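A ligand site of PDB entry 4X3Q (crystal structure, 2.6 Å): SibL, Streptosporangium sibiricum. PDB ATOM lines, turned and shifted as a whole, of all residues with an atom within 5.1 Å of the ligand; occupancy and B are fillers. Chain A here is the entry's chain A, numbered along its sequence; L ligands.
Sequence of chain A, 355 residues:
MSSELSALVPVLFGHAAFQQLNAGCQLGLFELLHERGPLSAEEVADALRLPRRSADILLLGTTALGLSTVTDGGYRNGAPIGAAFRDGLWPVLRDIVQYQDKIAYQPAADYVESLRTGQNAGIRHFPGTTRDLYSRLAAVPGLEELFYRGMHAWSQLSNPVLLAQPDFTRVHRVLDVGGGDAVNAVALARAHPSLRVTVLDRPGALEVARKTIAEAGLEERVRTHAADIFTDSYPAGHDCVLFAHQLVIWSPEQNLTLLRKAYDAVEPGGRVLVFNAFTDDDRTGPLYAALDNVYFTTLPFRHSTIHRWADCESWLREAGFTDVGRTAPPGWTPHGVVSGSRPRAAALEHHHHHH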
ATOM      1  N   TYR A 134      -5.263 -30.472  18.156  1.00  0.00           N
ATOM      2  CA  TYR A 134      -4.204 -29.948  17.286  1.00  0.00           C
ATOM      3  C   TYR A 134      -3.297 -28.994  18.038  1.00  0.00           C
ATOM      4  O   TYR A 134      -2.075 -29.099  17.926  1.00  0.00           O
ATOM      5  CB  TYR A 134      -4.842 -29.288  16.059  1.00  0.00           C
ATOM      6  CG  TYR A 134      -5.920 -30.186  15.519  1.00  0.00           C
ATOM      7  CD1 TYR A 134      -5.606 -31.295  14.739  1.00  0.00           C
ATOM      8  CD2 TYR A 134      -7.249 -29.980  15.875  1.00  0.00           C
ATOM      9  CE1 TYR A 134      -6.588 -32.144  14.273  1.00  0.00           C
ATOM     10  CE2 TYR A 134      -8.245 -30.820  15.411  1.00  0.00           C
ATOM     11  CZ  TYR A 134      -7.901 -31.901  14.611  1.00  0.00           C
ATOM     12  OH  TYR A 134      -8.895 -32.726  14.172  1.00  0.00           O
ATOM     13  N   PHE A 147       1.590 -37.424  14.458  1.00  0.00           N
ATOM     14  CA  PHE A 147       0.215 -37.185  14.084  1.00  0.00           C
ATOM     15  C   PHE A 147       0.103 -36.976  12.574  1.00  0.00           C
ATOM     16  O   PHE A 147      -0.799 -37.524  11.935  1.00  0.00           O
ATOM     17  CB  PHE A 147      -0.374 -35.990  14.828  1.00  0.00           C
ATOM     18  CG  PHE A 147      -1.768 -35.682  14.417  1.00  0.00           C
ATOM     19  CD1 PHE A 147      -2.837 -36.358  15.007  1.00  0.00           C
ATOM     20  CD2 PHE A 147      -2.040 -34.763  13.400  1.00  0.00           C
ATOM     21  CE1 PHE A 147      -4.134 -36.093  14.628  1.00  0.00           C
ATOM     22  CE2 PHE A 147      -3.343 -34.496  13.013  1.00  0.00           C
ATOM     23  CZ  PHE A 147      -4.386 -35.165  13.622  1.00  0.00           C
ATOM     24  N   TYR A 148       0.966 -36.149  11.994  1.00  0.00           N
ATOM     25  CA  TYR A 148       0.834 -35.880  10.577  1.00  0.00           C
ATOM     26  C   TYR A 148       1.272 -37.070   9.734  1.00  0.00           C
ATOM     27  O   TYR A 148       0.759 -37.252   8.623  1.00  0.00           O
ATOM     28  CB  TYR A 148       1.563 -34.588  10.178  1.00  0.00           C
ATOM     29  CG  TYR A 148       0.731 -33.417  10.658  1.00  0.00           C
ATOM     30  CD1 TYR A 148      -0.505 -33.156  10.088  1.00  0.00           C
ATOM     31  CD2 TYR A 148       1.127 -32.672  11.749  1.00  0.00           C
ATOM     32  CE1 TYR A 148      -1.305 -32.128  10.567  1.00  0.00           C
ATOM     33  CE2 TYR A 148       0.354 -31.666  12.242  1.00  0.00           C
ATOM     34  CZ  TYR A 148      -0.874 -31.380  11.656  1.00  0.00           C
ATOM     35  OH  TYR A 148      -1.642 -30.346  12.164  1.00  0.00           O
ATOM     36  N   MET A 151      -2.118 -38.588   9.516  1.00  0.00           N
ATOM     37  CA  MET A 151      -3.026 -37.850   8.646  1.00  0.00           C
ATOM     38  C   MET A 151      -2.638 -37.954   7.184  1.00  0.00           C
ATOM     39  O   MET A 151      -3.504 -38.161   6.322  1.00  0.00           O
ATOM     40  CB  MET A 151      -3.099 -36.386   9.058  1.00  0.00           C
ATOM     41  CG  MET A 151      -4.008 -36.171  10.231  1.00  0.00           C
ATOM     42  SD  MET A 151      -5.841 -36.831   9.908  1.00  0.00           S
ATOM     43  CE  MET A 151      -6.217 -35.918   8.225  1.00  0.00           C
ATOM     44  N   HIS A 152      -1.343 -37.824   6.918  1.00  0.00           N
ATOM     45  CA  HIS A 152      -0.798 -37.989   5.578  1.00  0.00           C
ATOM     46  C   HIS A 152      -1.351 -39.274   4.961  1.00  0.00           C
ATOM     47  O   HIS A 152      -1.928 -39.259   3.874  1.00  0.00           O
ATOM     48  CB  HIS A 152       0.723 -38.065   5.635  1.00  0.00           C
ATOM     49  CG  HIS A 152       1.416 -37.948   4.309  1.00  0.00           C
ATOM     50  ND1 HIS A 152       1.969 -36.767   3.861  1.00  0.00           N
ATOM     51  CD2 HIS A 152       1.589 -38.851   3.318  1.00  0.00           C
ATOM     52  CE1 HIS A 152       2.516 -36.966   2.667  1.00  0.00           C
ATOM     53  NE2 HIS A 152       2.284 -38.223   2.317  1.00  0.00           N
ATOM     54  N   SER A 155      -5.175 -39.433   4.234  1.00  0.00           N
ATOM     55  CA  SER A 155      -5.467 -38.695   3.018  1.00  0.00           C
ATOM     56  C   SER A 155      -4.995 -39.431   1.731  1.00  0.00           C
ATOM     57  O   SER A 155      -5.668 -39.376   0.714  1.00  0.00           O
ATOM     58  CB  SER A 155      -4.862 -37.297   3.112  1.00  0.00           C
ATOM     59  OG  SER A 155      -5.702 -36.458   3.871  1.00  0.00           O
ATOM     60  N   ASP A 176      -6.013 -24.024   0.904  1.00  0.00           N
ATOM     61  CA  ASP A 176      -6.110 -25.266   1.637  1.00  0.00           C
ATOM     62  C   ASP A 176      -6.335 -24.964   3.123  1.00  0.00           C
ATOM     63  O   ASP A 176      -5.366 -24.933   3.883  1.00  0.00           O
ATOM     64  CB  ASP A 176      -4.804 -26.057   1.446  1.00  0.00           C
ATOM     65  CG  ASP A 176      -4.926 -27.532   1.754  1.00  0.00           C
ATOM     66  OD1 ASP A 176      -5.999 -27.997   2.181  1.00  0.00           O
ATOM     67  OD2 ASP A 176      -3.906 -28.245   1.560  1.00  0.00           O
ATOM     68  N   GLY A 178      -6.572 -25.347   6.824  1.00  0.00           N
ATOM     69  CA  GLY A 178      -6.187 -26.425   7.708  1.00  0.00           C
ATOM     70  C   GLY A 178      -5.557 -27.556   6.919  1.00  0.00           C
ATOM     71  O   GLY A 178      -5.807 -28.738   7.177  1.00  0.00           O
ATOM     72  N   GLY A 179      -4.686 -27.201   5.986  1.00  0.00           N
ATOM     73  CA  GLY A 179      -4.114 -28.171   5.066  1.00  0.00           C
ATOM     74  C   GLY A 179      -3.093 -29.117   5.703  1.00  0.00           C
ATOM     75  O   GLY A 179      -2.520 -29.968   5.024  1.00  0.00           O
ATOM     76  N   GLY A 180      -2.832 -28.950   6.999  1.00  0.00           N
ATOM     77  CA  GLY A 180      -1.956 -29.868   7.705  1.00  0.00           C
ATOM     78  C   GLY A 180      -0.546 -29.930   7.143  1.00  0.00           C
ATOM     79  O   GLY A 180       0.121 -28.894   6.991  1.00  0.00           O
ATOM     80  N   ASP A 181      -0.087 -31.153   6.845  1.00  0.00           N
ATOM     81  CA  ASP A 181       1.269 -31.364   6.337  1.00  0.00           C
ATOM     82  C   ASP A 181       1.367 -31.214   4.818  1.00  0.00           C
ATOM     83  O   ASP A 181       2.386 -31.571   4.240  1.00  0.00           O
ATOM     84  CB  ASP A 181       1.789 -32.747   6.748  1.00  0.00           C
ATOM     85  CG  ASP A 181       1.293 -33.867   5.833  1.00  0.00           C
ATOM     86  OD1 ASP A 181       0.172 -33.736   5.276  1.00  0.00           O
ATOM     87  OD2 ASP A 181       2.018 -34.866   5.651  1.00  0.00           O
ATOM     88  N   VAL A 183      -0.172 -32.756   2.419  1.00  0.00           N
ATOM     89  CA  VAL A 183      -0.286 -33.994   1.656  1.00  0.00           C
ATOM     90  C   VAL A 183      -1.222 -33.806   0.447  1.00  0.00           C
ATOM     91  O   VAL A 183      -0.930 -34.265  -0.657  1.00  0.00           O
ATOM     92  CB  VAL A 183      -0.807 -35.155   2.559  1.00  0.00           C
ATOM     93  CG1 VAL A 183      -2.093 -34.770   3.264  1.00  0.00           C
ATOM     94  CG2 VAL A 183      -1.000 -36.450   1.759  1.00  0.00           C
ATOM     95  N   ASN A 184      -2.343 -33.125   0.665  1.00  0.00           N
ATOM     96  CA  ASN A 184      -3.366 -32.972  -0.366  1.00  0.00           C
ATOM     97  C   ASN A 184      -3.039 -31.872  -1.359  1.00  0.00           C
ATOM     98  O   ASN A 184      -3.409 -31.959  -2.540  1.00  0.00           O
ATOM     99  CB  ASN A 184      -4.736 -32.746   0.298  1.00  0.00           C
ATOM    100  CG  ASN A 184      -5.205 -33.960   1.085  1.00  0.00           C
ATOM    101  OD1 ASN A 184      -4.995 -35.095   0.666  1.00  0.00           O
ATOM    102  ND2 ASN A 184      -5.818 -33.733   2.233  1.00  0.00           N
ATOM    103  N   LEU A 200      -2.831 -23.364   4.569  1.00  0.00           N
ATOM    104  CA  LEU A 200      -3.092 -22.574   5.763  1.00  0.00           C
ATOM    105  C   LEU A 200      -3.236 -23.453   7.001  1.00  0.00           C
ATOM    106  O   LEU A 200      -4.082 -24.347   7.026  1.00  0.00           O
ATOM    107  CB  LEU A 200      -4.369 -21.744   5.565  1.00  0.00           C
ATOM    108  CG  LEU A 200      -4.730 -20.598   6.531  1.00  0.00           C
ATOM    109  CD1 LEU A 200      -5.660 -19.605   5.843  1.00  0.00           C
ATOM    110  CD2 LEU A 200      -5.378 -21.143   7.806  1.00  0.00           C
ATOM    111  N   ASP A 201      -2.444 -23.178   8.038  1.00  0.00           N
ATOM    112  CA  ASP A 201      -2.506 -23.982   9.238  1.00  0.00           C
ATOM    113  C   ASP A 201      -1.726 -23.346  10.403  1.00  0.00           C
ATOM    114  O   ASP A 201      -1.194 -22.244  10.293  1.00  0.00           O
ATOM    115  CB  ASP A 201      -1.970 -25.396   8.985  1.00  0.00           C
ATOM    116  CG  ASP A 201      -2.747 -26.459   9.761  1.00  0.00           C
ATOM    117  OD1 ASP A 201      -2.618 -26.493  11.007  1.00  0.00           O
ATOM    118  OD2 ASP A 201      -3.444 -27.275   9.128  1.00  0.00           O
ATOM    119  N   ARG A 202      -1.710 -24.039  11.537  1.00  0.00           N
ATOM    120  CA  ARG A 202      -0.891 -23.629  12.668  1.00  0.00           C
ATOM    121  C   ARG A 202       0.565 -23.721  12.244  1.00  0.00           C
ATOM    122  O   ARG A 202       0.921 -24.516  11.361  1.00  0.00           O
ATOM    123  CB  ARG A 202      -1.154 -24.513  13.896  1.00  0.00           C
ATOM    124  CG  ARG A 202      -2.636 -24.700  14.235  1.00  0.00           C
ATOM    125  CD  ARG A 202      -2.898 -26.038  14.939  1.00  0.00           C
ATOM    126  NE  ARG A 202      -1.670 -26.565  15.504  1.00  0.00           N
ATOM    127  CZ  ARG A 202      -1.029 -27.664  15.112  1.00  0.00           C
ATOM    128  NH1 ARG A 202      -1.536 -28.449  14.165  1.00  0.00           N
ATOM    129  NH2 ARG A 202       0.104 -27.989  15.713  1.00  0.00           N
ATOM    130  N   ALA A 205       2.163 -27.247  12.261  1.00  0.00           N
ATOM    131  CA  ALA A 205       1.842 -28.087  11.106  1.00  0.00           C
ATOM    132  C   ALA A 205       2.688 -27.697   9.877  1.00  0.00           C
ATOM    133  O   ALA A 205       3.186 -28.553   9.115  1.00  0.00           O
ATOM    134  CB  ALA A 205       0.364 -27.986  10.774  1.00  0.00           C
ATOM    135  N   ALA A 227      -1.949 -19.138  10.019  1.00  0.00           N
ATOM    136  CA  ALA A 227      -3.108 -18.363  10.401  1.00  0.00           C
ATOM    137  C   ALA A 227      -3.972 -19.234  11.256  1.00  0.00           C
ATOM    138  O   ALA A 227      -3.855 -20.454  11.230  1.00  0.00           O
ATOM    139  CB  ALA A 227      -3.872 -17.887   9.187  1.00  0.00           C
ATOM    140  N   ASP A 228      -4.858 -18.583  12.016  1.00  0.00           N
ATOM    141  CA  ASP A 228      -5.885 -19.274  12.725  1.00  0.00           C
ATOM    142  C   ASP A 228      -7.113 -19.315  11.821  1.00  0.00           C
ATOM    143  O   ASP A 228      -7.544 -18.271  11.340  1.00  0.00           O
ATOM    144  CB  ASP A 228      -6.202 -18.576  14.037  1.00  0.00           C
ATOM    145  CG  ASP A 228      -7.242 -19.345  14.858  1.00  0.00           C
ATOM    146  OD1 ASP A 228      -8.439 -19.298  14.513  1.00  0.00           O
ATOM    147  OD2 ASP A 228      -6.837 -20.024  15.802  1.00  0.00           O
ATOM    148  N   ILE A 229      -7.657 -20.495  11.552  1.00  0.00           N
ATOM    149  CA  ILE A 229      -8.769 -20.600  10.595  1.00  0.00           C
ATOM    150  C   ILE A 229     -10.031 -19.848  11.053  1.00  0.00           C
ATOM    151  O   ILE A 229     -10.908 -19.564  10.241  1.00  0.00           O
ATOM    152  CB  ILE A 229      -9.154 -22.064  10.301  1.00  0.00           C
ATOM    153  CG1 ILE A 229      -9.809 -22.712  11.536  1.00  0.00           C
ATOM    154  CG2 ILE A 229      -7.961 -22.869   9.836  1.00  0.00           C
ATOM    155  CD1 ILE A 229     -10.178 -24.155  11.337  1.00  0.00           C
ATOM    156  N   PHE A 230     -10.139 -19.538  12.358  1.00  0.00           N
ATOM    157  CA  PHE A 230     -11.286 -18.769  12.857  1.00  0.00           C
ATOM    158  C   PHE A 230     -11.066 -17.235  12.985  1.00  0.00           C
ATOM    159  O   PHE A 230     -11.937 -16.459  12.583  1.00  0.00           O
ATOM    160  CB  PHE A 230     -11.753 -19.314  14.221  1.00  0.00           C
ATOM    161  CG  PHE A 230     -12.474 -20.637  14.130  1.00  0.00           C
ATOM    162  CD1 PHE A 230     -13.790 -20.705  13.676  1.00  0.00           C
ATOM    163  CD2 PHE A 230     -11.840 -21.819  14.501  1.00  0.00           C
ATOM    164  CE1 PHE A 230     -14.463 -21.921  13.580  1.00  0.00           C
ATOM    165  CE2 PHE A 230     -12.514 -23.048  14.416  1.00  0.00           C
ATOM    166  CZ  PHE A 230     -13.835 -23.092  13.946  1.00  0.00           C
ATOM    167  N   ALA A 244     -10.377 -29.909   3.626  1.00  0.00           N
ATOM    168  CA  ALA A 244     -10.150 -31.353   3.612  1.00  0.00           C
ATOM    169  C   ALA A 244      -9.997 -31.900   5.039  1.00  0.00           C
ATOM    170  O   ALA A 244      -9.082 -31.516   5.766  1.00  0.00           O
ATOM    171  CB  ALA A 244      -8.919 -31.691   2.779  1.00  0.00           C
ATOM    172  N   HIS A 245     -10.934 -32.788   5.420  1.00  0.00           N
ATOM    173  CA  HIS A 245     -10.939 -33.427   6.761  1.00  0.00           C
ATOM    174  C   HIS A 245     -10.918 -32.356   7.824  1.00  0.00           C
ATOM    175  O   HIS A 245     -10.118 -32.402   8.742  1.00  0.00           O
ATOM    176  CB  HIS A 245      -9.743 -34.360   6.940  1.00  0.00           C
ATOM    177  CG  HIS A 245      -9.675 -35.444   5.908  1.00  0.00           C
ATOM    178  ND1 HIS A 245      -8.573 -35.631   5.102  1.00  0.00           N
ATOM    179  CD2 HIS A 245     -10.582 -36.372   5.536  1.00  0.00           C
ATOM    180  CE1 HIS A 245      -8.806 -36.637   4.285  1.00  0.00           C
ATOM    181  NE2 HIS A 245     -10.012 -37.107   4.533  1.00  0.00           N
ATOM    182  N   GLN A 246     -11.795 -31.375   7.646  1.00  0.00           N
ATOM    183  CA  GLN A 246     -11.742 -30.157   8.439  1.00  0.00           C
ATOM    184  C   GLN A 246     -13.066 -29.915   9.135  1.00  0.00           C
ATOM    185  O   GLN A 246     -13.124 -29.736  10.349  1.00  0.00           O
ATOM    186  CB  GLN A 246     -11.379 -28.964   7.538  1.00  0.00           C
ATOM    187  CG  GLN A 246     -11.165 -27.656   8.286  1.00  0.00           C
ATOM    188  CD  GLN A 246     -10.028 -27.769   9.260  1.00  0.00           C
ATOM    189  OE1 GLN A 246     -10.169 -27.429  10.429  1.00  0.00           O
ATOM    190  NE2 GLN A 246      -8.879 -28.226   8.792  1.00  0.00           N
ATOM    191  N   ILE A 249     -14.387 -31.620  12.297  1.00  0.00           N
ATOM    192  CA  ILE A 249     -13.935 -31.179  13.609  1.00  0.00           C
ATOM    193  C   ILE A 249     -14.932 -30.295  14.359  1.00  0.00           C
ATOM    194  O   ILE A 249     -14.987 -30.304  15.587  1.00  0.00           O
ATOM    195  CB  ILE A 249     -12.612 -30.415  13.452  1.00  0.00           C
ATOM    196  CG1 ILE A 249     -11.639 -31.246  12.602  1.00  0.00           C
ATOM    197  CG2 ILE A 249     -12.027 -30.026  14.842  1.00  0.00           C
ATOM    198  CD1 ILE A 249     -10.386 -30.517  12.224  1.00  0.00           C
ATOM    199  N   TRP A 250     -15.695 -29.500  13.631  1.00  0.00           N
ATOM    200  CA  TRP A 250     -16.419 -28.414  14.280  1.00  0.00           C
ATOM    201  C   TRP A 250     -17.928 -28.597  14.280  1.00  0.00           C
ATOM    202  O   TRP A 250     -18.468 -29.423  13.547  1.00  0.00           O
ATOM    203  CB  TRP A 250     -16.040 -27.088  13.611  1.00  0.00           C
ATOM    204  CG  TRP A 250     -14.528 -26.973  13.324  1.00  0.00           C
ATOM    205  CD1 TRP A 250     -13.917 -27.029  12.107  1.00  0.00           C
ATOM    206  CD2 TRP A 250     -13.474 -26.820  14.285  1.00  0.00           C
ATOM    207  NE1 TRP A 250     -12.545 -26.893  12.232  1.00  0.00           N
ATOM    208  CE2 TRP A 250     -12.246 -26.773  13.566  1.00  0.00           C
ATOM    209  CE3 TRP A 250     -13.434 -26.711  15.693  1.00  0.00           C
ATOM    210  CZ2 TRP A 250     -10.998 -26.616  14.193  1.00  0.00           C
ATOM    211  CZ3 TRP A 250     -12.193 -26.574  16.322  1.00  0.00           C
ATOM    212  CH2 TRP A 250     -10.995 -26.530  15.561  1.00  0.00           C
HETATM  213  N1  LIG L   1      -6.001 -31.089   5.650  1.00  0.00           N
HETATM  214  C1  LIG L   1      -5.085 -32.014   6.220  1.00  0.00           C
HETATM  215  C2  LIG L   1      -5.116 -31.997   7.743  1.00  0.00           C
HETATM  216  C3  LIG L   1      -6.467 -32.336   8.363  1.00  0.00           C
HETATM  217  S1  LIG L   1      -6.333 -32.501  10.135  1.00  0.00           S
HETATM  218  C4  LIG L   1      -5.458 -33.387   5.715  1.00  0.00           C
HETATM  219  O1  LIG L   1      -4.663 -34.364   5.855  1.00  0.00           O
HETATM  220  O2  LIG L   1      -6.558 -33.541   5.151  1.00  0.00           O
HETATM  221  C5  LIG L   1      -7.000 -30.989  10.820  1.00  0.00           C
HETATM  222  C6  LIG L   1      -6.080 -29.791  10.562  1.00  0.00           C
HETATM  223  O3  LIG L   1      -6.749 -28.544  10.927  1.00  0.00           O
HETATM  224  C7  LIG L   1      -4.799 -29.847  11.457  1.00  0.00           C
HETATM  225  O4  LIG L   1      -3.642 -29.674  10.664  1.00  0.00           O
HETATM  226  C8  LIG L   1      -4.935 -28.663  12.395  1.00  0.00           C
HETATM  227  O5  LIG L   1      -3.630 -28.105  12.729  1.00  0.00           O
HETATM  228  C9  LIG L   1      -5.773 -27.711  11.549  1.00  0.00           C
HETATM  229  N2  LIG L   1      -6.339 -26.739  12.374  1.00  0.00           N
HETATM  230  C10 LIG L   1      -7.265 -26.934  13.316  1.00  0.00           C
HETATM  231  N3  LIG L   1      -7.609 -25.802  13.944  1.00  0.00           N
HETATM  232  C11 LIG L   1      -6.833 -24.834  13.357  1.00  0.00           C
HETATM  233  C12 LIG L   1      -6.715 -23.460  13.574  1.00  0.00           C
HETATM  234  N4  LIG L   1      -7.433 -22.813  14.523  1.00  0.00           N
HETATM  235  N5  LIG L   1      -5.865 -22.773  12.798  1.00  0.00           N
HETATM  236  C13 LIG L   1      -5.116 -23.427  11.888  1.00  0.00           C
HETATM  237  N6  LIG L   1      -5.149 -24.730  11.603  1.00  0.00           N
HETATM  238  C14 LIG L   1      -6.035 -25.410  12.384  1.00  0.00           C
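An oxygen (O5) of the ligand lies within hydrogen-bond range of the guanidinium group (NH1) of Arg 202.
OD1 of Asp 201 lies within hydrogen-bond range of O5 of the ligand.
OH of Tyr 148 is in hydrogen-bond range of O4 of the ligand, 2.6 Å away.
The backbone carbonyl oxygen of Gly 178 lies within hydrogen-bond range of a nitrogen (N1) of the ligand (2.8 Å).
ND1 of His 245 lies within hydrogen-bond range of O2 of the ligand, 2.9 Å away.
ND2 of Asn 184 lies within hydrogen-bond range of O2 of the ligand (3.0 Å).
An oxygen (O3) of the ligand lies within hydrogen-bond range of the side-chain amide nitrogen (NE2) of Gln 246.
The side-chain hydroxyl (OG) of Ser 155 is in hydrogen-bond range of an oxygen (O1) of the ligand.
O of Ala 244 lies within hydrogen-bond range of N1 of the ligand (3.1 Å).
The side-chain carboxylate (OD2) of Asp 228 is in hydrogen-bond range of a nitrogen (N4) of the ligand.
N of Ile 229 sits at hydrogen-bond distance from N5 of the ligand (3.2 Å).
The side-chain carboxylate (OD1) of Asp 201 lies within salt-bridge range of the guanidinium group (NH1) of Arg 202, 3.9 Å away.
NH1 of Arg 202 is in hydrogen-bond range of OH of Tyr 148, 2.8 Å away.
The guanidinium group (NH2) of Arg 202 lies within hydrogen-bond range of the backbone carbonyl oxygen (O) of Tyr 134 (3.3 Å).
O of Asp 201 is in hydrogen-bond range of N of Ala 227 (3.2 Å).
The backbone NH of Gly 180 lies within hydrogen-bond range of the side-chain carboxylate of Asp 201 (2.8 Å).
The backbone carbonyl oxygen (O) of Leu 200 lies within hydrogen-bond range of the backbone NH (N) of Gly 178, 2.7 Å away.
The side-chain amide oxygen (OE1) of Gln 246 is in hydrogen-bond range of the indole nitrogen (NE1) of Trp 250, at 3.0 Å.
The side-chain carboxylate of Asp 228 is in hydrogen-bond range of the backbone NH of Phe 230, 2.8 Å away.
The backbone carbonyl oxygen (O) of Ala 227 sits close to a nitrogen (N5) of the ligand, 3.4 Å away.
Merely in contact with the ligand: Met 151, Gly 180, Gly 179, Trp 250, Tyr 134, Val 183 and Ile 249.
Within 4 Å of the ligand: Tyr 134, Tyr 148, Met 151, Ser 155, Gly 178, Gly 179, Gly 180, Val 183, Asn 184, Asp 201, Arg 202, Ala 227, Asp 228, Ile 229, Ala 244, His 245, Gln 246, Ile 249 and Trp 250.
Along chain A the residues within 4 Å of the ligand span positions 134 to 250.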
